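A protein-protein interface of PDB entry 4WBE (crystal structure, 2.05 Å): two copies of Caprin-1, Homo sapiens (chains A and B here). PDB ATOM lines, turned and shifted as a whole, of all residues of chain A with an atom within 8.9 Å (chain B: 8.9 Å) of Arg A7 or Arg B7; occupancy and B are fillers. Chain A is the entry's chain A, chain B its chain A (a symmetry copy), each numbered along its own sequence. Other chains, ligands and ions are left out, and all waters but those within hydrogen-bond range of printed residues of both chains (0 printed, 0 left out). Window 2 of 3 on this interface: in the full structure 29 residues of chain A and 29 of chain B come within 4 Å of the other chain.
OE2 of Glu A11 is in salt-bridge range of NE of Arg B14, at 2.6 Å. NE of Arg A14 is in salt-bridge range of OE2 of Glu B11, at 2.6 Å.
The backbone carbonyl oxygen of Glu A3 lies close to the guanidinium group of Arg A7 (3.3 Å). The side-chain amide nitrogen of Gln A4 sits at hydrogen-bond distance from the side-chain carboxylate of Glu A8, at 3.5 Å. The backbone carbonyl oxygen of Glu B3 sits close to the guanidinium group of Arg B7 (3.3 Å). NE2 of Gln B4 lies within hydrogen-bond range of OE2 of Glu B8, 3.5 Å away.
Among the printed residues, merely in contact across the chains: Trp A84 with Gln B12, Gln A12 with Trp B84, Glu A11 with Glu B11, Trp A84 with Glu B8, Glu A8 with Trp B84, Arg A7 with Arg B7, Trp A84 with Glu B11 and Glu A11 with Trp B84.
Arg A7 touches just one residue of chain B: Arg B7. Printed residues of chain B within 4 Å of Arg A14: Glu B11 (2.6 Å). Of the printed residues of chain B, Gln A12 touches Trp B84 (3.3 Å). Printed residues of chain A within 4 Å of Gln B12: Trp A84. Printed residues of chain B within 4 Å of Trp A84: Glu B8, Glu B11 and Gln B12. Printed residues of chain A within 4 Å of Arg B14: Glu A11 (2.6 Å). Arg B1 touches none of the printed residues of chain A. Ala B10 touches none of the printed residues of chain A. The nearest residue of chain B that does not touch Arg A7 is Glu B11 (5.9 Å). The nearest printed residue of chain B that does not touch Gln A12 is Glu B11 (5.8 Å).
Hydrophobic or aromatic side chains of chain A that line the printed part of chain B: Trp A84. Among the printed residues, 10 pairs touch across the chains.
Arg B7 touches its own counterpart, Arg A7. Glu A8 touches Trp B84, and with the chains exchanged Trp A84 touches Glu B8. Glu B11 touches its own counterpart, Glu A11. Glu A11 touches Trp B84, and with the chains exchanged Trp A84 touches Glu B11. Positions printed for both chains: 1, 2, 3, 4, 5, 6, 7, 8, 9, 10, 11, 12, 13, 14 and 84.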
ATOM      1  N   ARG A   1     -22.562  -1.204  -9.804  1.00  0.00           N
ATOM      2  CA  ARG A   1     -22.957  -2.281 -10.701  1.00  0.00           C
ATOM      3  C   ARG A   1     -24.479  -2.352 -10.850  1.00  0.00           C
ATOM      4  O   ARG A   1     -24.996  -2.369 -11.969  1.00  0.00           O
ATOM      5  CB  ARG A   1     -22.394  -3.611 -10.193  1.00  0.00           C
ATOM      6  CG  ARG A   1     -23.004  -4.850 -10.825  1.00  0.00           C
ATOM      7  CD  ARG A   1     -22.831  -4.877 -12.333  1.00  0.00           C
ATOM      8  NE  ARG A   1     -23.590  -5.969 -12.937  1.00  0.00           N
ATOM      9  CZ  ARG A   1     -24.850  -5.865 -13.345  1.00  0.00           C
ATOM     10  NH1 ARG A   1     -25.496  -4.713 -13.222  1.00  0.00           N
ATOM     11  NH2 ARG A   1     -25.461  -6.911 -13.881  1.00  0.00           N
ATOM     12  N   ARG A   2     -25.197  -2.381  -9.730  1.00  0.00           N
ATOM     13  CA  ARG A   2     -26.650  -2.262  -9.791  1.00  0.00           C
ATOM     14  C   ARG A   2     -27.012  -0.788  -9.813  1.00  0.00           C
ATOM     15  O   ARG A   2     -28.060  -0.403 -10.326  1.00  0.00           O
ATOM     16  CB  ARG A   2     -27.369  -2.949  -8.632  1.00  0.00           C
ATOM     17  CG  ARG A   2     -28.870  -3.041  -8.914  1.00  0.00           C
ATOM     18  CD  ARG A   2     -29.658  -3.791  -7.869  1.00  0.00           C
ATOM     19  NE  ARG A   2     -29.875  -2.979  -6.681  1.00  0.00           N
ATOM     20  CZ  ARG A   2     -30.294  -3.463  -5.520  1.00  0.00           C
ATOM     21  NH1 ARG A   2     -30.544  -4.755  -5.399  1.00  0.00           N
ATOM     22  NH2 ARG A   2     -30.465  -2.655  -4.485  1.00  0.00           N
ATOM     23  N   GLU A   3     -26.139   0.034  -9.241  1.00  0.00           N
ATOM     24  CA  GLU A   3     -26.279   1.479  -9.349  1.00  0.00           C
ATOM     25  C   GLU A   3     -26.164   1.892 -10.814  1.00  0.00           C
ATOM     26  O   GLU A   3     -26.694   2.924 -11.215  1.00  0.00           O
ATOM     27  CB  GLU A   3     -25.238   2.191  -8.484  1.00  0.00           C
ATOM     28  CG  GLU A   3     -25.536   2.100  -6.992  1.00  0.00           C
ATOM     29  CD  GLU A   3     -24.450   2.718  -6.131  1.00  0.00           C
ATOM     30  OE1 GLU A   3     -23.389   3.081  -6.682  1.00  0.00           O
ATOM     31  OE2 GLU A   3     -24.654   2.830  -4.903  1.00  0.00           O
ATOM     32  N   GLN A   4     -25.466   1.078 -11.600  1.00  0.00           N
ATOM     33  CA  GLN A   4     -25.350   1.300 -13.036  1.00  0.00           C
ATOM     34  C   GLN A   4     -26.707   1.092 -13.706  1.00  0.00           C
ATOM     35  O   GLN A   4     -27.174   1.946 -14.465  1.00  0.00           O
ATOM     36  CB  GLN A   4     -24.308   0.353 -13.633  1.00  0.00           C
ATOM     37  CG  GLN A   4     -24.128   0.475 -15.141  1.00  0.00           C
ATOM     38  CD  GLN A   4     -23.227  -0.610 -15.717  1.00  0.00           C
ATOM     39  OE1 GLN A   4     -22.724  -1.469 -14.988  1.00  0.00           O
ATOM     40  NE2 GLN A   4     -23.013  -0.568 -17.029  1.00  0.00           N
ATOM     41  N   LEU A   5     -27.330  -0.051 -13.433  1.00  0.00           N
ATOM     42  CA  LEU A   5     -28.661  -0.338 -13.962  1.00  0.00           C
ATOM     43  C   LEU A   5     -29.665   0.726 -13.524  1.00  0.00           C
ATOM     44  O   LEU A   5     -30.509   1.154 -14.318  1.00  0.00           O
ATOM     45  CB  LEU A   5     -29.137  -1.729 -13.533  1.00  0.00           C
ATOM     46  CG  LEU A   5     -28.454  -2.934 -14.193  1.00  0.00           C
ATOM     47  CD1 LEU A   5     -29.066  -4.251 -13.714  1.00  0.00           C
ATOM     48  CD2 LEU A   5     -28.491  -2.843 -15.710  1.00  0.00           C
ATOM     49  N   MET A   6     -29.566   1.161 -12.268  1.00  0.00           N
ATOM     50  CA  MET A   6     -30.480   2.189 -11.764  1.00  0.00           C
ATOM     51  C   MET A   6     -30.310   3.526 -12.481  1.00  0.00           C
ATOM     52  O   MET A   6     -31.287   4.217 -12.753  1.00  0.00           O
ATOM     53  CB  MET A   6     -30.337   2.384 -10.248  1.00  0.00           C
ATOM     54  CG  MET A   6     -30.717   1.166  -9.413  1.00  0.00           C
ATOM     55  SD  MET A   6     -32.369   0.531  -9.803  1.00  0.00           S
ATOM     56  CE  MET A   6     -31.899  -0.956 -10.650  1.00  0.00           C
ATOM     57  N   ARG A   7     -29.065   3.892 -12.764  1.00  0.00           N
ATOM     58  CA  ARG A   7     -28.794   5.125 -13.490  1.00  0.00           C
ATOM     59  C   ARG A   7     -29.306   5.045 -14.927  1.00  0.00           C
ATOM     60  O   ARG A   7     -29.848   6.010 -15.459  1.00  0.00           O
ATOM     61  CB  ARG A   7     -27.293   5.466 -13.430  1.00  0.00           C
ATOM     62  CG  ARG A   7     -26.853   5.918 -12.029  1.00  0.00           C
ATOM     63  CD  ARG A   7     -25.477   6.589 -11.983  1.00  0.00           C
ATOM     64  NE  ARG A   7     -24.385   5.725 -12.429  1.00  0.00           N
ATOM     65  CZ  ARG A   7     -23.721   4.887 -11.637  1.00  0.00           C
ATOM     66  NH1 ARG A   7     -24.043   4.781 -10.354  1.00  0.00           N
ATOM     67  NH2 ARG A   7     -22.737   4.148 -12.132  1.00  0.00           N
ATOM     68  N   GLU A   8     -29.127   3.888 -15.550  1.00  0.00           N
ATOM     69  CA  GLU A   8     -29.614   3.673 -16.904  1.00  0.00           C
ATOM     70  C   GLU A   8     -31.147   3.744 -16.978  1.00  0.00           C
ATOM     71  O   GLU A   8     -31.712   4.307 -17.923  1.00  0.00           O
ATOM     72  CB  GLU A   8     -29.032   2.371 -17.466  1.00  0.00           C
ATOM     73  CG  GLU A   8     -27.511   2.459 -17.683  1.00  0.00           C
ATOM     74  CD  GLU A   8     -26.881   1.162 -18.159  1.00  0.00           C
ATOM     75  OE1 GLU A   8     -27.599   0.142 -18.258  1.00  0.00           O
ATOM     76  OE2 GLU A   8     -25.662   1.165 -18.444  1.00  0.00           O
ATOM     77  N   GLU A   9     -31.813   3.191 -15.972  1.00  0.00           N
ATOM     78  CA  GLU A   9     -33.263   3.265 -15.895  1.00  0.00           C
ATOM     79  C   GLU A   9     -33.720   4.709 -15.733  1.00  0.00           C
ATOM     80  O   GLU A   9     -34.647   5.155 -16.403  1.00  0.00           O
ATOM     81  CB  GLU A   9     -33.772   2.453 -14.702  1.00  0.00           C
ATOM     82  CG  GLU A   9     -35.287   2.417 -14.605  1.00  0.00           C
ATOM     83  CD  GLU A   9     -35.897   1.549 -15.689  1.00  0.00           C
ATOM     84  OE1 GLU A   9     -35.492   0.371 -15.791  1.00  0.00           O
ATOM     85  OE2 GLU A   9     -36.759   2.042 -16.453  1.00  0.00           O
ATOM     86  N   ALA A  10     -33.063   5.435 -14.835  1.00  0.00           N
ATOM     87  CA  ALA A  10     -33.415   6.830 -14.597  1.00  0.00           C
ATOM     88  C   ALA A  10     -33.243   7.679 -15.854  1.00  0.00           C
ATOM     89  O   ALA A  10     -34.017   8.597 -16.098  1.00  0.00           O
ATOM     90  CB  ALA A  10     -32.607   7.403 -13.433  1.00  0.00           C
ATOM     91  N   GLU A  11     -32.216   7.374 -16.641  1.00  0.00           N
ATOM     92  CA  GLU A  11     -31.973   8.116 -17.867  1.00  0.00           C
ATOM     93  C   GLU A  11     -33.050   7.812 -18.907  1.00  0.00           C
ATOM     94  O   GLU A  11     -33.569   8.718 -19.552  1.00  0.00           O
ATOM     95  CB  GLU A  11     -30.562   7.858 -18.400  1.00  0.00           C
ATOM     96  CG  GLU A  11     -30.148   8.868 -19.458  1.00  0.00           C
ATOM     97  CD  GLU A  11     -28.667   8.805 -19.782  1.00  0.00           C
ATOM     98  OE1 GLU A  11     -27.991   7.873 -19.299  1.00  0.00           O
ATOM     99  OE2 GLU A  11     -28.176   9.716 -20.477  1.00  0.00           O
ATOM    100  N   GLN A  12     -33.387   6.536 -19.063  1.00  0.00           N
ATOM    101  CA  GLN A  12     -34.475   6.151 -19.955  1.00  0.00           C
ATOM    102  C   GLN A  12     -35.802   6.790 -19.568  1.00  0.00           C
ATOM    103  O   GLN A  12     -36.524   7.290 -20.436  1.00  0.00           O
ATOM    104  CB  GLN A  12     -34.651   4.632 -19.974  1.00  0.00           C
ATOM    105  CG  GLN A  12     -33.558   3.875 -20.691  1.00  0.00           C
ATOM    106  CD  GLN A  12     -33.560   2.400 -20.339  1.00  0.00           C
ATOM    107  OE1 GLN A  12     -34.315   1.957 -19.473  1.00  0.00           O
ATOM    108  NE2 GLN A  12     -32.715   1.629 -21.017  1.00  0.00           N
ATOM    109  N   LYS A  13     -36.113   6.772 -18.272  1.00  0.00           N
ATOM    110  CA  LYS A  13     -37.343   7.372 -17.744  1.00  0.00           C
ATOM    111  C   LYS A  13     -37.362   8.870 -17.988  1.00  0.00           C
ATOM    112  O   LYS A  13     -38.417   9.463 -18.220  1.00  0.00           O
ATOM    113  CB  LYS A  13     -37.483   7.081 -16.247  1.00  0.00           C
ATOM    114  CG  LYS A  13     -37.757   5.613 -15.916  1.00  0.00           C
ATOM    115  CD  LYS A  13     -39.152   5.188 -16.370  1.00  0.00           C
ATOM    116  CE  LYS A  13     -39.453   3.738 -15.971  1.00  0.00           C
ATOM    117  NZ  LYS A  13     -40.869   3.370 -16.275  1.00  0.00           N
ATOM    118  N   ARG A  14     -36.183   9.477 -17.904  1.00  0.00           N
ATOM    119  CA  ARG A  14     -36.021  10.887 -18.204  1.00  0.00           C
ATOM    120  C   ARG A  14     -36.329  11.173 -19.680  1.00  0.00           C
ATOM    121  O   ARG A  14     -37.000  12.159 -20.003  1.00  0.00           O
ATOM    122  CB  ARG A  14     -34.594  11.315 -17.848  1.00  0.00           C
ATOM    123  CG  ARG A  14     -34.253  12.719 -18.264  1.00  0.00           C
ATOM    124  CD  ARG A  14     -33.177  13.325 -17.373  1.00  0.00           C
ATOM    125  NE  ARG A  14     -32.968  12.534 -16.160  1.00  0.00           N
ATOM    126  CZ  ARG A  14     -33.028  13.023 -14.925  1.00  0.00           C
ATOM    127  NH1 ARG A  14     -33.282  14.309 -14.730  1.00  0.00           N
ATOM    128  NH2 ARG A  14     -32.827  12.225 -13.885  1.00  0.00           N
ATOM    129  N   TRP A  84     -33.001  19.577 -19.371  1.00  0.00           N
ATOM    130  CA  TRP A  84     -32.413  18.917 -18.209  1.00  0.00           C
ATOM    131  C   TRP A  84     -32.745  19.664 -16.919  1.00  0.00           C
ATOM    132  O   TRP A  84     -33.106  19.051 -15.906  1.00  0.00           O
ATOM    133  CB  TRP A  84     -30.895  18.774 -18.362  1.00  0.00           C
ATOM    134  CG  TRP A  84     -30.300  17.894 -17.309  1.00  0.00           C
ATOM    135  CD1 TRP A  84     -30.206  16.527 -17.339  1.00  0.00           C
ATOM    136  CD2 TRP A  84     -29.735  18.307 -16.064  1.00  0.00           C
ATOM    137  NE1 TRP A  84     -29.612  16.070 -16.188  1.00  0.00           N
ATOM    138  CE2 TRP A  84     -29.314  17.143 -15.388  1.00  0.00           C
ATOM    139  CE3 TRP A  84     -29.535  19.548 -15.457  1.00  0.00           C
ATOM    140  CZ2 TRP A  84     -28.708  17.186 -14.135  1.00  0.00           C
ATOM    141  CZ3 TRP A  84     -28.936  19.589 -14.214  1.00  0.00           C
ATOM    142  CH2 TRP A  84     -28.529  18.417 -13.565  1.00  0.00           C
ATOM    143  N   ARG B   1     -18.499  12.793  -6.869  1.00  0.00           N
ATOM    144  CA  ARG B   1     -18.756  14.220  -6.739  1.00  0.00           C
ATOM    145  C   ARG B   1     -18.477  14.959  -8.050  1.00  0.00           C
ATOM    146  O   ARG B   1     -19.326  15.709  -8.537  1.00  0.00           O
ATOM    147  CB  ARG B   1     -17.915  14.796  -5.597  1.00  0.00           C
ATOM    148  CG  ARG B   1     -17.819  16.312  -5.571  1.00  0.00           C
ATOM    149  CD  ARG B   1     -19.180  16.977  -5.458  1.00  0.00           C
ATOM    150  NE  ARG B   1     -19.082  18.423  -5.631  1.00  0.00           N
ATOM    151  CZ  ARG B   1     -19.168  19.041  -6.804  1.00  0.00           C
ATOM    152  NH1 ARG B   1     -19.361  18.340  -7.913  1.00  0.00           N
ATOM    153  NH2 ARG B   1     -19.066  20.361  -6.866  1.00  0.00           N
ATOM    154  N   ARG B   2     -17.299  14.741  -8.630  1.00  0.00           N
ATOM    155  CA  ARG B   2     -17.036  15.260  -9.968  1.00  0.00           C
ATOM    156  C   ARG B   2     -17.558  14.261 -10.984  1.00  0.00           C
ATOM    157  O   ARG B   2     -17.902  14.623 -12.107  1.00  0.00           O
ATOM    158  CB  ARG B   2     -15.559  15.541 -10.236  1.00  0.00           C
ATOM    159  CG  ARG B   2     -15.394  16.350 -11.524  1.00  0.00           C
ATOM    160  CD  ARG B   2     -13.974  16.761 -11.827  1.00  0.00           C
ATOM    161  NE  ARG B   2     -13.201  15.650 -12.362  1.00  0.00           N
ATOM    162  CZ  ARG B   2     -11.879  15.649 -12.461  1.00  0.00           C
ATOM    163  NH1 ARG B   2     -11.190  16.706 -12.066  1.00  0.00           N
ATOM    164  NH2 ARG B   2     -11.250  14.595 -12.958  1.00  0.00           N
ATOM    165  N   GLU B   3     -17.604  12.994 -10.584  1.00  0.00           N
ATOM    166  CA  GLU B   3     -18.244  11.969 -11.394  1.00  0.00           C
ATOM    167  C   GLU B   3     -19.729  12.291 -11.539  1.00  0.00           C
ATOM    168  O   GLU B   3     -20.365  11.884 -12.508  1.00  0.00           O
ATOM    169  CB  GLU B   3     -18.031  10.584 -10.784  1.00  0.00           C
ATOM    170  CG  GLU B   3     -16.605  10.070 -10.952  1.00  0.00           C
ATOM    171  CD  GLU B   3     -16.368   8.741 -10.258  1.00  0.00           C
ATOM    172  OE1 GLU B   3     -17.265   8.290  -9.514  1.00  0.00           O
ATOM    173  OE2 GLU B   3     -15.280   8.155 -10.447  1.00  0.00           O
ATOM    174  N   GLN B   4     -20.269  13.020 -10.567  1.00  0.00           N
ATOM    175  CA  GLN B   4     -21.652  13.479 -10.620  1.00  0.00           C
ATOM    176  C   GLN B   4     -21.818  14.504 -11.740  1.00  0.00           C
ATOM    177  O   GLN B   4     -22.713  14.381 -12.581  1.00  0.00           O
ATOM    178  CB  GLN B   4     -22.059  14.084  -9.276  1.00  0.00           C
ATOM    179  CG  GLN B   4     -23.480  14.628  -9.228  1.00  0.00           C
ATOM    180  CD  GLN B   4     -23.776  15.389  -7.941  1.00  0.00           C
ATOM    181  OE1 GLN B   4     -22.916  15.516  -7.067  1.00  0.00           O
ATOM    182  NE2 GLN B   4     -25.003  15.890  -7.818  1.00  0.00           N
ATOM    183  N   LEU B   5     -20.962  15.522 -11.739  1.00  0.00           N
ATOM    184  CA  LEU B   5     -20.978  16.532 -12.793  1.00  0.00           C
ATOM    185  C   LEU B   5     -20.769  15.895 -14.165  1.00  0.00           C
ATOM    186  O   LEU B   5     -21.430  16.274 -15.138  1.00  0.00           O
ATOM    187  CB  LEU B   5     -19.923  17.611 -12.540  1.00  0.00           C
ATOM    188  CG  LEU B   5     -20.190  18.594 -11.392  1.00  0.00           C
ATOM    189  CD1 LEU B   5     -19.084  19.646 -11.292  1.00  0.00           C
ATOM    190  CD2 LEU B   5     -21.553  19.254 -11.521  1.00  0.00           C
ATOM    191  N   MET B   6     -19.864  14.920 -14.240  1.00  0.00           N
ATOM    192  CA  MET B   6     -19.604  14.244 -15.513  1.00  0.00           C
ATOM    193  C   MET B   6     -20.816  13.465 -16.020  1.00  0.00           C
ATOM    194  O   MET B   6     -21.089  13.445 -17.217  1.00  0.00           O
ATOM    195  CB  MET B   6     -18.383  13.316 -15.427  1.00  0.00           C
ATOM    196  CG  MET B   6     -17.062  14.030 -15.157  1.00  0.00           C
ATOM    197  SD  MET B   6     -16.736  15.377 -16.325  1.00  0.00           S
ATOM    198  CE  MET B   6     -17.003  16.754 -15.237  1.00  0.00           C
ATOM    199  N   ARG B   7     -21.524  12.812 -15.107  1.00  0.00           N
ATOM    200  CA  ARG B   7     -22.727  12.079 -15.476  1.00  0.00           C
ATOM    201  C   ARG B   7     -23.832  13.027 -15.940  1.00  0.00           C
ATOM    202  O   ARG B   7     -24.553  12.740 -16.891  1.00  0.00           O
ATOM    203  CB  ARG B   7     -23.188  11.180 -14.314  1.00  0.00           C
ATOM    204  CG  ARG B   7     -22.246   9.986 -14.091  1.00  0.00           C
ATOM    205  CD  ARG B   7     -22.821   8.885 -13.195  1.00  0.00           C
ATOM    206  NE  ARG B   7     -23.139   9.334 -11.840  1.00  0.00           N
ATOM    207  CZ  ARG B   7     -22.272   9.349 -10.832  1.00  0.00           C
ATOM    208  NH1 ARG B   7     -21.018   8.956 -11.021  1.00  0.00           N
ATOM    209  NH2 ARG B   7     -22.657   9.767  -9.634  1.00  0.00           N
ATOM    210  N   GLU B   8     -23.960  14.156 -15.256  1.00  0.00           N
ATOM    211  CA  GLU B   8     -24.944  15.161 -15.631  1.00  0.00           C
ATOM    212  C   GLU B   8     -24.653  15.757 -17.017  1.00  0.00           C
ATOM    213  O   GLU B   8     -25.571  15.989 -17.813  1.00  0.00           O
ATOM    214  CB  GLU B   8     -25.061  16.214 -14.522  1.00  0.00           C
ATOM    215  CG  GLU B   8     -25.669  15.635 -13.232  1.00  0.00           C
ATOM    216  CD  GLU B   8     -25.725  16.624 -12.081  1.00  0.00           C
ATOM    217  OE1 GLU B   8     -25.221  17.759 -12.235  1.00  0.00           O
ATOM    218  OE2 GLU B   8     -26.281  16.266 -11.019  1.00  0.00           O
ATOM    219  N   GLU B   9     -23.378  15.983 -17.307  1.00  0.00           N
ATOM    220  CA  GLU B   9     -22.977  16.471 -18.616  1.00  0.00           C
ATOM    221  C   GLU B   9     -23.300  15.447 -19.695  1.00  0.00           C
ATOM    222  O   GLU B   9     -23.837  15.786 -20.746  1.00  0.00           O
ATOM    223  CB  GLU B   9     -21.472  16.750 -18.639  1.00  0.00           C
ATOM    224  CG  GLU B   9     -20.992  17.341 -19.953  1.00  0.00           C
ATOM    225  CD  GLU B   9     -21.445  18.780 -20.117  1.00  0.00           C
ATOM    226  OE1 GLU B   9     -21.162  19.588 -19.207  1.00  0.00           O
ATOM    227  OE2 GLU B   9     -22.100  19.101 -21.136  1.00  0.00           O
ATOM    228  N   ALA B  10     -22.966  14.189 -19.429  1.00  0.00           N
ATOM    229  CA  ALA B  10     -23.229  13.124 -20.389  1.00  0.00           C
ATOM    230  C   ALA B  10     -24.721  12.984 -20.683  1.00  0.00           C
ATOM    231  O   ALA B  10     -25.112  12.690 -21.807  1.00  0.00           O
ATOM    232  CB  ALA B  10     -22.638  11.800 -19.909  1.00  0.00           C
ATOM    233  N   GLU B  11     -25.548  13.181 -19.662  1.00  0.00           N
ATOM    234  CA  GLU B  11     -26.988  13.081 -19.841  1.00  0.00           C
ATOM    235  C   GLU B  11     -27.512  14.245 -20.682  1.00  0.00           C
ATOM    236  O   GLU B  11     -28.313  14.047 -21.590  1.00  0.00           O
ATOM    237  CB  GLU B  11     -27.707  12.968 -18.495  1.00  0.00           C
ATOM    238  CG  GLU B  11     -29.148  12.509 -18.645  1.00  0.00           C
ATOM    239  CD  GLU B  11     -29.780  12.116 -17.323  1.00  0.00           C
ATOM    240  OE1 GLU B  11     -29.149  12.347 -16.270  1.00  0.00           O
ATOM    241  OE2 GLU B  11     -30.881  11.533 -17.345  1.00  0.00           O
ATOM    242  N   GLN B  12     -27.051  15.455 -20.381  1.00  0.00           N
ATOM    243  CA  GLN B  12     -27.409  16.616 -21.188  1.00  0.00           C
ATOM    244  C   GLN B  12     -26.993  16.465 -22.646  1.00  0.00           C
ATOM    245  O   GLN B  12     -27.777  16.774 -23.548  1.00  0.00           O
ATOM    246  CB  GLN B  12     -26.770  17.886 -20.626  1.00  0.00           C
ATOM    247  CG  GLN B  12     -27.371  18.379 -19.330  1.00  0.00           C
ATOM    248  CD  GLN B  12     -26.468  19.370 -18.623  1.00  0.00           C
ATOM    249  OE1 GLN B  12     -25.338  19.611 -19.048  1.00  0.00           O
ATOM    250  NE2 GLN B  12     -26.967  19.955 -17.538  1.00  0.00           N
ATOM    251  N   LYS B  13     -25.766  15.991 -22.866  1.00  0.00           N
ATOM    252  CA  LYS B  13     -25.234  15.766 -24.214  1.00  0.00           C
ATOM    253  C   LYS B  13     -26.046  14.715 -24.947  1.00  0.00           C
ATOM    254  O   LYS B  13     -26.225  14.784 -26.165  1.00  0.00           O
ATOM    255  CB  LYS B  13     -23.764  15.343 -24.147  1.00  0.00           C
ATOM    256  CG  LYS B  13     -22.813  16.449 -23.684  1.00  0.00           C
ATOM    257  CD  LYS B  13     -22.692  17.557 -24.727  1.00  0.00           C
ATOM    258  CE  LYS B  13     -21.682  18.627 -24.293  1.00  0.00           C
ATOM    259  NZ  LYS B  13     -21.448  19.628 -25.376  1.00  0.00           N
ATOM    260  N   ARG B  14     -26.512  13.725 -24.193  1.00  0.00           N
ATOM    261  CA  ARG B  14     -27.384  12.696 -24.728  1.00  0.00           C
ATOM    262  C   ARG B  14     -28.722  13.293 -25.185  1.00  0.00           C
ATOM    263  O   ARG B  14     -29.235  12.943 -26.253  1.00  0.00           O
ATOM    264  CB  ARG B  14     -27.601  11.618 -23.661  1.00  0.00           C
ATOM    265  CG  ARG B  14     -28.617  10.577 -24.039  1.00  0.00           C
ATOM    266  CD  ARG B  14     -28.346   9.247 -23.346  1.00  0.00           C
ATOM    267  NE  ARG B  14     -27.012   9.210 -22.747  1.00  0.00           N
ATOM    268  CZ  ARG B  14     -26.107   8.267 -22.987  1.00  0.00           C
ATOM    269  NH1 ARG B  14     -26.389   7.269 -23.812  1.00  0.00           N
ATOM    270  NH2 ARG B  14     -24.920   8.321 -22.397  1.00  0.00           N
ATOM    271  N   TRP B  84     -32.664   5.219 -26.216  1.00  0.00           N
ATOM    272  CA  TRP B  84     -31.523   4.950 -25.346  1.00  0.00           C
ATOM    273  C   TRP B  84     -30.604   3.889 -25.946  1.00  0.00           C
ATOM    274  O   TRP B  84     -29.376   4.036 -25.939  1.00  0.00           O
ATOM    275  CB  TRP B  84     -31.981   4.524 -23.947  1.00  0.00           C
ATOM    276  CG  TRP B  84     -30.849   4.478 -22.971  1.00  0.00           C
ATOM    277  CD1 TRP B  84     -30.348   5.526 -22.242  1.00  0.00           C
ATOM    278  CD2 TRP B  84     -30.061   3.338 -22.625  1.00  0.00           C
ATOM    279  NE1 TRP B  84     -29.301   5.101 -21.464  1.00  0.00           N
ATOM    280  CE2 TRP B  84     -29.103   3.762 -21.681  1.00  0.00           C
ATOM    281  CE3 TRP B  84     -30.074   1.997 -23.014  1.00  0.00           C
ATOM    282  CZ2 TRP B  84     -28.168   2.892 -21.124  1.00  0.00           C
ATOM    283  CZ3 TRP B  84     -29.147   1.137 -22.462  1.00  0.00           C
ATOM    284  CH2 TRP B  84     -28.206   1.586 -21.528  1.00  0.00           C
